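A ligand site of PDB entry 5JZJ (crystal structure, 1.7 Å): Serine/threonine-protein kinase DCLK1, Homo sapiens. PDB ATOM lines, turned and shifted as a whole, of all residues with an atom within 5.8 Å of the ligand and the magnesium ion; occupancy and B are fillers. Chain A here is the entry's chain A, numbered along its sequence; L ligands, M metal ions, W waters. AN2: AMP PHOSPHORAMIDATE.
The backbone carbonyl oxygen (O) of Asp 159 sits at hydrogen-bond distance from the side-chain amide nitrogen (ND2) of Asn 164.
O of Asn 164 sits at hydrogen-bond distance from N of Gly 180, at 2.9 Å.
The side-chain carboxylate of Glu 163 is in salt-bridge range of the side-chain amino group of Lys 161, at 3.9 Å.
The side-chain amino group (NZ) of Lys 67 is in salt-bridge range of the side-chain carboxylate (OE2) of Glu 84 (3.0 Å).
The backbone NH of Asp 123 sits at hydrogen-bond distance from the side-chain carboxylate of Asp 120 (2.9 Å).
O of Gly 45 lies within hydrogen-bond range of N of Val 52 (3.0 Å).
The backbone NH of Ile 44 sits at hydrogen-bond distance from the backbone carbonyl oxygen of Val 52 (2.9 Å).
O of Ala 65 sits at hydrogen-bond distance from N of Met 113 (2.8 Å).
The magnesium ion is bound by OD2 of Asp 181 (2.1 Å), O1B of the ligand (2.1 Å), O1A of the ligand (2.1 Å), OD1 of Asn 164 (2.1 Å), water W1 (2.1 Å) and water W3 (2.2 Å).
The magnesium ion has six donor atoms within binding distance.
Within 4 Å of the magnesium ion: Asn 164 and Asp 181.
O of Glu 163 sits at hydrogen-bond distance from O3' of the ligand (2.6 Å).
The side-chain amino group (NZ) of Lys 67 lies within salt-bridge range of an oxygen (O2A) of the ligand.
An oxygen (O2') of the ligand lies within hydrogen-bond range of the side-chain carboxylate (OD2) of Asp 120, 2.7 Å away.
O of Glu 114 lies within hydrogen-bond range of N6 of the ligand (2.9 Å).
N of Ala 50 is in hydrogen-bond range of O2B of the ligand (3.0 Å).
The backbone NH (N) of Val 116 is in hydrogen-bond range of a nitrogen (N1) of the ligand, at 3.1 Å.
An oxygen (O2B) of the ligand lies within hydrogen-bond range of the backbone NH (N) of Phe 49 (3.4 Å).
CD1 of Ile 44 touches C2 of the ligand, 3.7 Å away.
Gly 45 touches the ligand.
O of Asp 46 touches C5' of the ligand, at 3.5 Å.
Gly 47 touches the ligand (CA to O2B, 3.1 Å).
N of Asn 48 touches O2B of the ligand, at 3.6 Å.
Val 52 touches the ligand.
Ala 65 touches the ligand (CB to N6, 3.7 Å).
Val 97 touches the ligand (CG1 to N6, 3.6 Å).
Met 113 touches the ligand.
Leu 115 touches the ligand.
Leu 166 touches the ligand (CD1 to C6, 3.3 Å).
Hydrophobic or aromatic side chains within 4 Å of the ligand: Ile 44, Ala 50, Val 52, Ala 65, Val 97, Met 113, Leu 115, Val 116 and Leu 166.
20 residues have an atom within 4 Å of the ligand: Ile 44, Gly 45, Asp 46, Gly 47, Asn 48, Phe 49, Ala 50, Val 52, Ala 65, Lys 67, Val 97, Met 113, Glu 114, Leu 115, Val 116, Asp 120, Glu 163, Asn 164, Leu 166 and Asp 181.
Water W3 bridges the side-chain carboxylate of Glu 163 and the side-chain amide nitrogen of Asn 164.
Water W1 bridges O3' of the ligand and OE2 of Glu 163.
Water W4 lies within hydrogen-bond range of an oxygen (O2A) of the ligand (2.7 Å) and the backbone NH (N) of Asp 181 (2.9 Å).
Water W7 lies within hydrogen-bond range of O2' of the ligand (2.7 Å) and O of Ile 44 (2.7 Å).
Water W9 lies within hydrogen-bond range of OD1 of Asp 181 (2.6 Å), NZ of Lys 67 (2.7 Å), OE1 of Glu 84 (2.7 Å) and N3B of the ligand (2.8 Å).
Water W8 bridges N of Asp 46 (3.2 Å) and O2' of the ligand (3.4 Å).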
ATOM      1  N   ILE A  44      13.516   1.269  -4.002  1.00  0.00           N
ATOM      2  CA  ILE A  44      12.465   0.562  -4.745  1.00  0.00           C
ATOM      3  C   ILE A  44      12.160  -0.789  -4.134  1.00  0.00           C
ATOM      4  O   ILE A  44      11.182  -1.430  -4.496  1.00  0.00           O
ATOM      5  CB  ILE A  44      12.832   0.425  -6.233  1.00  0.00           C
ATOM      6  CG1 ILE A  44      14.235  -0.223  -6.400  1.00  0.00           C
ATOM      7  CG2 ILE A  44      12.691   1.751  -6.917  1.00  0.00           C
ATOM      8  CD1 ILE A  44      14.564  -0.681  -7.779  1.00  0.00           C
ATOM      9  N   GLY A  45      13.014  -1.201  -3.222  1.00  0.00           N
ATOM     10  CA  GLY A  45      12.852  -2.461  -2.541  1.00  0.00           C
ATOM     11  C   GLY A  45      13.791  -2.573  -1.368  1.00  0.00           C
ATOM     12  O   GLY A  45      14.758  -1.808  -1.259  1.00  0.00           O
ATOM     13  N   ASP A  46      13.484  -3.511  -0.488  1.00  0.00           N
ATOM     14  CA  ASP A  46      14.276  -3.757   0.706  1.00  0.00           C
ATOM     15  C   ASP A  46      14.189  -5.234   1.083  1.00  0.00           C
ATOM     16  O   ASP A  46      13.292  -5.942   0.599  1.00  0.00           O
ATOM     17  CB  ASP A  46      13.779  -2.868   1.871  1.00  0.00           C
ATOM     18  CG  ASP A  46      14.873  -2.271   2.727  1.00  0.00           C
ATOM     19  OD1 ASP A  46      15.598  -3.052   3.387  1.00  0.00           O
ATOM     20  OD2 ASP A  46      14.967  -1.035   2.788  1.00  0.00           O
ATOM     21  N   GLY A  47      15.094  -5.663   1.923  1.00  0.00           N
ATOM     22  CA  GLY A  47      15.148  -7.023   2.438  1.00  0.00           C
ATOM     23  C   GLY A  47      15.795  -6.970   3.800  1.00  0.00           C
ATOM     24  O   GLY A  47      16.086  -5.876   4.297  1.00  0.00           O
ATOM     25  N   ASN A  48      16.048  -8.130   4.398  1.00  0.00           N
ATOM     26  CA  ASN A  48      16.703  -8.210   5.713  1.00  0.00           C
ATOM     27  C   ASN A  48      18.121  -7.674   5.686  1.00  0.00           C
ATOM     28  O   ASN A  48      18.584  -7.150   6.702  1.00  0.00           O
ATOM     29  CB  ASN A  48      16.743  -9.654   6.199  1.00  0.00           C
ATOM     30  CG  ASN A  48      15.420 -10.185   6.647  1.00  0.00           C
ATOM     31  OD1 ASN A  48      14.761  -9.615   7.542  1.00  0.00           O
ATOM     32  ND2 ASN A  48      15.013 -11.319   6.079  1.00  0.00           N
ATOM     33  N   PHE A  49      18.820  -7.843   4.548  1.00  0.00           N
ATOM     34  CA  PHE A  49      20.225  -7.508   4.432  1.00  0.00           C
ATOM     35  C   PHE A  49      20.511  -6.363   3.471  1.00  0.00           C
ATOM     36  O   PHE A  49      21.589  -5.757   3.568  1.00  0.00           O
ATOM     37  CB  PHE A  49      21.001  -8.759   3.968  1.00  0.00           C
ATOM     38  N   ALA A  50      19.604  -6.086   2.531  1.00  0.00           N
ATOM     39  CA  ALA A  50      19.908  -5.069   1.541  1.00  0.00           C
ATOM     40  C   ALA A  50      18.846  -4.019   1.362  1.00  0.00           C
ATOM     41  O   ALA A  50      17.663  -4.251   1.590  1.00  0.00           O
ATOM     42  CB  ALA A  50      20.184  -5.747   0.194  1.00  0.00           C
ATOM     43  N   VAL A  51      19.303  -2.851   0.884  1.00  0.00           N
ATOM     44  CA  VAL A  51      18.460  -1.741   0.452  1.00  0.00           C
ATOM     45  C   VAL A  51      18.771  -1.588  -1.033  1.00  0.00           C
ATOM     46  O   VAL A  51      19.936  -1.512  -1.410  1.00  0.00           O
ATOM     47  CB  VAL A  51      18.651  -0.432   1.275  1.00  0.00           C
ATOM     48  CG1 VAL A  51      17.802   0.702   0.699  1.00  0.00           C
ATOM     49  CG2 VAL A  51      18.299  -0.666   2.735  1.00  0.00           C
ATOM     50  N   VAL A  52      17.733  -1.579  -1.849  1.00  0.00           N
ATOM     51  CA  VAL A  52      17.855  -1.482  -3.310  1.00  0.00           C
ATOM     52  C   VAL A  52      17.244  -0.178  -3.761  1.00  0.00           C
ATOM     53  O   VAL A  52      16.088   0.104  -3.424  1.00  0.00           O
ATOM     54  CB  VAL A  52      17.214  -2.692  -4.035  1.00  0.00           C
ATOM     55  CG1 VAL A  52      17.354  -2.561  -5.549  1.00  0.00           C
ATOM     56  CG2 VAL A  52      17.815  -4.014  -3.546  1.00  0.00           C
ATOM     57  N   ALA A  65      19.707  -0.692 -11.075  1.00  0.00           N
ATOM     58  CA  ALA A  65      19.385  -0.839  -9.666  1.00  0.00           C
ATOM     59  C   ALA A  65      20.696  -0.782  -8.894  1.00  0.00           C
ATOM     60  O   ALA A  65      21.728  -1.304  -9.360  1.00  0.00           O
ATOM     61  CB  ALA A  65      18.649  -2.153  -9.403  1.00  0.00           C
ATOM     62  N   LYS A  67      22.102  -2.046  -5.465  1.00  0.00           N
ATOM     63  CA  LYS A  67      21.862  -2.870  -4.280  1.00  0.00           C
ATOM     64  C   LYS A  67      22.979  -2.593  -3.243  1.00  0.00           C
ATOM     65  O   LYS A  67      24.164  -2.723  -3.538  1.00  0.00           O
ATOM     66  CB  LYS A  67      21.774  -4.352  -4.646  1.00  0.00           C
ATOM     67  CG  LYS A  67      21.588  -5.252  -3.430  1.00  0.00           C
ATOM     68  CD  LYS A  67      21.164  -6.640  -3.847  1.00  0.00           C
ATOM     69  CE  LYS A  67      21.352  -7.620  -2.713  1.00  0.00           C
ATOM     70  NZ  LYS A  67      20.822  -8.978  -3.090  1.00  0.00           N
ATOM     71  N   GLU A  84      27.947 -13.812  -2.102  1.00  0.00           N
ATOM     72  CA  GLU A  84      27.092 -13.417  -3.244  1.00  0.00           C
ATOM     73  C   GLU A  84      27.830 -12.974  -4.537  1.00  0.00           C
ATOM     74  O   GLU A  84      27.491 -13.487  -5.596  1.00  0.00           O
ATOM     75  CB  GLU A  84      26.122 -12.325  -2.809  1.00  0.00           C
ATOM     76  CG  GLU A  84      25.025 -12.031  -3.818  1.00  0.00           C
ATOM     77  CD  GLU A  84      23.884 -11.217  -3.233  1.00  0.00           C
ATOM     78  OE1 GLU A  84      23.730 -11.228  -1.986  1.00  0.00           O
ATOM     79  OE2 GLU A  84      23.134 -10.579  -4.000  1.00  0.00           O
ATOM     80  N   VAL A  97      18.933 -11.787 -12.962  1.00  0.00           N
ATOM     81  CA  VAL A  97      19.317 -10.374 -12.872  1.00  0.00           C
ATOM     82  C   VAL A  97      20.832 -10.247 -13.112  1.00  0.00           C
ATOM     83  O   VAL A  97      21.626 -10.895 -12.427  1.00  0.00           O
ATOM     84  CB  VAL A  97      18.897  -9.701 -11.527  1.00  0.00           C
ATOM     85  CG1 VAL A  97      19.320  -8.235 -11.493  1.00  0.00           C
ATOM     86  CG2 VAL A  97      17.398  -9.825 -11.275  1.00  0.00           C
ATOM     87  N   MET A 113      23.197  -3.299 -10.666  1.00  0.00           N
ATOM     88  CA  MET A 113      22.550  -4.411 -11.355  1.00  0.00           C
ATOM     89  C   MET A 113      21.544  -3.941 -12.365  1.00  0.00           C
ATOM     90  O   MET A 113      21.126  -2.781 -12.355  1.00  0.00           O
ATOM     91  CB  MET A 113      21.859  -5.340 -10.322  1.00  0.00           C
ATOM     92  CG  MET A 113      22.576  -5.358  -8.972  1.00  0.00           C
ATOM     93  SD  MET A 113      22.106  -6.708  -7.897  1.00  0.00           S
ATOM     94  CE  MET A 113      20.352  -6.562  -7.940  1.00  0.00           C
ATOM     95  N   GLU A 114      21.128  -4.851 -13.235  1.00  0.00           N
ATOM     96  CA  GLU A 114      20.073  -4.623 -14.213  1.00  0.00           C
ATOM     97  C   GLU A 114      18.810  -4.216 -13.444  1.00  0.00           C
ATOM     98  O   GLU A 114      18.475  -4.846 -12.444  1.00  0.00           O
ATOM     99  CB  GLU A 114      19.850  -5.961 -14.944  1.00  0.00           C
ATOM    100  CG  GLU A 114      18.622  -6.060 -15.793  1.00  0.00           C
ATOM    101  CD  GLU A 114      18.499  -7.415 -16.468  1.00  0.00           C
ATOM    102  OE1 GLU A 114      17.767  -7.500 -17.477  1.00  0.00           O
ATOM    103  OE2 GLU A 114      19.159  -8.384 -16.020  1.00  0.00           O
ATOM    104  N   LEU A 115      18.128  -3.174 -13.898  1.00  0.00           N
ATOM    105  CA  LEU A 115      16.905  -2.755 -13.209  1.00  0.00           C
ATOM    106  C   LEU A 115      15.724  -3.494 -13.788  1.00  0.00           C
ATOM    107  O   LEU A 115      15.555  -3.538 -14.993  1.00  0.00           O
ATOM    108  CB  LEU A 115      16.688  -1.231 -13.309  1.00  0.00           C
ATOM    109  CG  LEU A 115      15.365  -0.681 -12.744  1.00  0.00           C
ATOM    110  CD1 LEU A 115      15.293  -0.804 -11.261  1.00  0.00           C
ATOM    111  CD2 LEU A 115      15.175   0.782 -13.139  1.00  0.00           C
ATOM    112  N   VAL A 116      14.901  -4.069 -12.911  1.00  0.00           N
ATOM    113  CA  VAL A 116      13.697  -4.741 -13.364  1.00  0.00           C
ATOM    114  C   VAL A 116      12.544  -3.891 -12.828  1.00  0.00           C
ATOM    115  O   VAL A 116      12.250  -3.861 -11.636  1.00  0.00           O
ATOM    116  CB  VAL A 116      13.677  -6.241 -12.954  1.00  0.00           C
ATOM    117  CG1 VAL A 116      12.486  -6.933 -13.584  1.00  0.00           C
ATOM    118  CG2 VAL A 116      14.962  -6.924 -13.390  1.00  0.00           C
ATOM    119  N   LYS A 117      11.952  -3.120 -13.738  1.00  0.00           N
ATOM    120  CA  LYS A 117      10.917  -2.129 -13.417  1.00  0.00           C
ATOM    121  C   LYS A 117       9.592  -2.697 -12.864  1.00  0.00           C
ATOM    122  O   LYS A 117       8.925  -1.970 -12.128  1.00  0.00           O
ATOM    123  CB  LYS A 117      10.614  -1.265 -14.656  1.00  0.00           C
ATOM    124  CG  LYS A 117      11.772  -0.343 -15.039  1.00  0.00           C
ATOM    125  CD  LYS A 117      11.308   1.015 -15.559  1.00  0.00           C
ATOM    126  CE  LYS A 117      11.233   2.069 -14.470  1.00  0.00           C
ATOM    127  NZ  LYS A 117      11.173   3.444 -15.035  1.00  0.00           N
ATOM    128  N   GLY A 119       8.925  -4.745 -10.451  1.00  0.00           N
ATOM    129  CA  GLY A 119       8.927  -5.106  -9.030  1.00  0.00           C
ATOM    130  C   GLY A 119       9.069  -6.611  -8.824  1.00  0.00           C
ATOM    131  O   GLY A 119       9.493  -7.327  -9.746  1.00  0.00           O
ATOM    132  N   ASP A 120       8.722  -7.097  -7.628  1.00  0.00           N
ATOM    133  CA  ASP A 120       8.915  -8.524  -7.375  1.00  0.00           C
ATOM    134  C   ASP A 120       7.610  -9.306  -7.429  1.00  0.00           C
ATOM    135  O   ASP A 120       6.498  -8.750  -7.362  1.00  0.00           O
ATOM    136  CB  ASP A 120       9.676  -8.750  -6.068  1.00  0.00           C
ATOM    137  CG  ASP A 120       8.911  -8.340  -4.825  1.00  0.00           C
ATOM    138  OD1 ASP A 120       7.809  -8.870  -4.617  1.00  0.00           O
ATOM    139  OD2 ASP A 120       9.467  -7.584  -4.013  1.00  0.00           O
ATOM    140  N   ASP A 123       4.938  -9.028  -4.382  1.00  0.00           N
ATOM    141  CA  ASP A 123       3.956  -7.947  -4.526  1.00  0.00           C
ATOM    142  C   ASP A 123       2.955  -8.236  -5.642  1.00  0.00           C
ATOM    143  O   ASP A 123       1.768  -7.912  -5.489  1.00  0.00           O
ATOM    144  CB  ASP A 123       4.658  -6.606  -4.746  1.00  0.00           C
ATOM    145  CG  ASP A 123       5.368  -6.111  -3.509  1.00  0.00           C
ATOM    146  OD1 ASP A 123       4.918  -6.437  -2.386  1.00  0.00           O
ATOM    147  OD2 ASP A 123       6.327  -5.336  -3.644  1.00  0.00           O
ATOM    148  N   ASP A 159      17.343 -20.008  -2.420  1.00  0.00           N
ATOM    149  CA  ASP A 159      16.454 -19.005  -1.864  1.00  0.00           C
ATOM    150  C   ASP A 159      15.453 -18.578  -2.906  1.00  0.00           C
ATOM    151  O   ASP A 159      15.089 -17.399  -2.981  1.00  0.00           O
ATOM    152  CB  ASP A 159      17.267 -17.804  -1.321  1.00  0.00           C
ATOM    153  CG  ASP A 159      16.571 -16.968  -0.244  1.00  0.00           C
ATOM    154  OD1 ASP A 159      15.585 -17.469   0.365  1.00  0.00           O
ATOM    155  OD2 ASP A 159      17.013 -15.843   0.001  1.00  0.00           O
ATOM    156  N   LYS A 161      12.020 -17.952  -4.175  1.00  0.00           N
ATOM    157  CA  LYS A 161      10.712 -17.615  -3.609  1.00  0.00           C
ATOM    158  C   LYS A 161      10.255 -16.317  -4.269  1.00  0.00           C
ATOM    159  O   LYS A 161      11.081 -15.636  -4.872  1.00  0.00           O
ATOM    160  CB  LYS A 161      10.768 -17.483  -2.078  1.00  0.00           C
ATOM    161  CG  LYS A 161      11.830 -16.505  -1.589  1.00  0.00           C
ATOM    162  CD  LYS A 161      11.946 -16.621  -0.061  1.00  0.00           C
ATOM    163  CE  LYS A 161      12.834 -15.556   0.500  1.00  0.00           C
ATOM    164  NZ  LYS A 161      13.377 -15.949   1.814  1.00  0.00           N
ATOM    165  N   GLU A 163       9.583 -13.201  -3.406  1.00  0.00           N
ATOM    166  CA  GLU A 163      10.249 -11.903  -3.179  1.00  0.00           C
ATOM    167  C   GLU A 163      11.605 -11.795  -3.922  1.00  0.00           C
ATOM    168  O   GLU A 163      12.107 -10.682  -4.124  1.00  0.00           O
ATOM    169  CB  GLU A 163      10.418 -11.672  -1.681  1.00  0.00           C
ATOM    170  CG  GLU A 163      11.404 -12.597  -1.006  1.00  0.00           C
ATOM    171  CD  GLU A 163      11.329 -12.521   0.501  1.00  0.00           C
ATOM    172  OE1 GLU A 163      10.243 -12.839   1.044  1.00  0.00           O
ATOM    173  OE2 GLU A 163      12.353 -12.200   1.138  1.00  0.00           O
ATOM    174  N   ASN A 164      12.181 -12.938  -4.316  1.00  0.00           N
ATOM    175  CA  ASN A 164      13.441 -13.013  -5.047  1.00  0.00           C
ATOM    176  C   ASN A 164      13.250 -13.235  -6.552  1.00  0.00           C
ATOM    177  O   ASN A 164      14.245 -13.469  -7.261  1.00  0.00           O
ATOM    178  CB  ASN A 164      14.353 -14.066  -4.443  1.00  0.00           C
ATOM    179  CG  ASN A 164      14.818 -13.622  -3.081  1.00  0.00           C
ATOM    180  OD1 ASN A 164      14.818 -12.404  -2.783  1.00  0.00           O
ATOM    181  ND2 ASN A 164      15.244 -14.554  -2.259  1.00  0.00           N
ATOM    182  N   LEU A 166      11.839 -11.276  -9.967  1.00  0.00           N
ATOM    183  CA  LEU A 166      11.476  -9.948 -10.465  1.00  0.00           C
ATOM    184  C   LEU A 166      10.704 -10.054 -11.755  1.00  0.00           C
ATOM    185  O   LEU A 166      10.955 -10.961 -12.548  1.00  0.00           O
ATOM    186  CB  LEU A 166      12.720  -9.103 -10.664  1.00  0.00           C
ATOM    187  CG  LEU A 166      13.649  -8.991  -9.428  1.00  0.00           C
ATOM    188  CD1 LEU A 166      14.791  -8.126  -9.736  1.00  0.00           C
ATOM    189  CD2 LEU A 166      12.914  -8.463  -8.209  1.00  0.00           C
ATOM    190  N   GLY A 180      16.622 -13.307  -8.883  1.00  0.00           N
ATOM    191  CA  GLY A 180      17.612 -12.506  -8.184  1.00  0.00           C
ATOM    192  C   GLY A 180      18.009 -13.097  -6.850  1.00  0.00           C
ATOM    193  O   GLY A 180      17.691 -14.249  -6.548  1.00  0.00           O
ATOM    194  N   ASP A 181      18.661 -12.275  -6.017  1.00  0.00           N
ATOM    195  CA  ASP A 181      19.096 -12.548  -4.648  1.00  0.00           C
ATOM    196  C   ASP A 181      19.887 -13.857  -4.518  1.00  0.00           C
ATOM    197  O   ASP A 181      19.352 -14.894  -4.070  1.00  0.00           O
ATOM    198  CB  ASP A 181      17.914 -12.564  -3.681  1.00  0.00           C
ATOM    199  CG  ASP A 181      18.295 -12.552  -2.201  1.00  0.00           C
ATOM    200  OD1 ASP A 181      19.498 -12.707  -1.899  1.00  0.00           O
ATOM    201  OD2 ASP A 181      17.410 -12.286  -1.357  1.00  0.00           O
HETATM  202  N3B AN2 L   1      18.878 -10.144   0.327  1.00  0.00           N
HETATM  203  PB  AN2 L   1      17.582  -9.171   0.226  1.00  0.00           P
HETATM  204  O2B AN2 L   1      17.787  -8.170   1.295  1.00  0.00           O
HETATM  205  O1B AN2 L   1      16.351  -9.992   0.255  1.00  0.00           O
HETATM  206  O3A AN2 L   1      17.812  -8.415  -1.214  1.00  0.00           O
HETATM  207  PA  AN2 L   1      17.170  -8.683  -2.671  1.00  0.00           P
HETATM  208  O1A AN2 L   1      16.132  -9.750  -2.626  1.00  0.00           O
HETATM  209  O2A AN2 L   1      18.246  -8.739  -3.677  1.00  0.00           O
HETATM  210  O5' AN2 L   1      16.343  -7.318  -2.889  1.00  0.00           O
HETATM  211  C5' AN2 L   1      15.201  -6.997  -2.076  1.00  0.00           C
HETATM  212  C4' AN2 L   1      14.060  -6.439  -2.945  1.00  0.00           C
HETATM  213  O4' AN2 L   1      14.547  -5.384  -3.801  1.00  0.00           O
HETATM  214  C3' AN2 L   1      13.536  -7.483  -3.909  1.00  0.00           C
HETATM  215  O3' AN2 L   1      12.548  -8.285  -3.250  1.00  0.00           O
HETATM  216  C2' AN2 L   1      12.882  -6.576  -4.983  1.00  0.00           C
HETATM  217  O2' AN2 L   1      11.642  -6.023  -4.488  1.00  0.00           O
HETATM  218  C1' AN2 L   1      13.905  -5.440  -5.079  1.00  0.00           C
HETATM  219  N9  AN2 L   1      14.960  -5.688  -6.091  1.00  0.00           N
HETATM  220  C8  AN2 L   1      16.109  -6.366  -5.926  1.00  0.00           C
HETATM  221  N7  AN2 L   1      16.802  -6.321  -7.060  1.00  0.00           N
HETATM  222  C5  AN2 L   1      16.126  -5.575  -7.930  1.00  0.00           C
HETATM  223  C4  AN2 L   1      14.990  -5.174  -7.312  1.00  0.00           C
HETATM  224  N3  AN2 L   1      14.086  -4.392  -7.962  1.00  0.00           N
HETATM  225  C2  AN2 L   1      14.339  -4.027  -9.273  1.00  0.00           C
HETATM  226  N1  AN2 L   1      15.490  -4.474  -9.901  1.00  0.00           N
HETATM  227  C6  AN2 L   1      16.366  -5.222  -9.220  1.00  0.00           C
HETATM  228  N6  AN2 L   1      17.473  -5.648  -9.824  1.00  0.00           N
HETATM  229 MG    MG M   1      15.661 -11.216  -1.246  1.00  0.00          MG
HETATM  230  O   HOH W   1      13.749 -10.286  -1.162  1.00  0.00           O
HETATM  231  O   HOH W   2      15.394 -10.406   2.810  1.00  0.00           O
HETATM  232  O   HOH W   3      14.893 -12.578   0.238  1.00  0.00           O
HETATM  233  O   HOH W   4      18.547  -9.375  -6.234  1.00  0.00           O
HETATM  234  O   HOH W   5      11.577  -3.487  -7.490  1.00  0.00           O
HETATM  235  O   HOH W   6      15.317  -9.978  -5.415  1.00  0.00           O
HETATM  236  O   HOH W   7      10.209  -3.880  -5.145  1.00  0.00           O
HETATM  237  O   HOH W   8      10.748  -4.803  -1.410  1.00  0.00           O
HETATM  238  O   HOH W   9      21.149 -10.836  -1.173  1.00  0.00           O
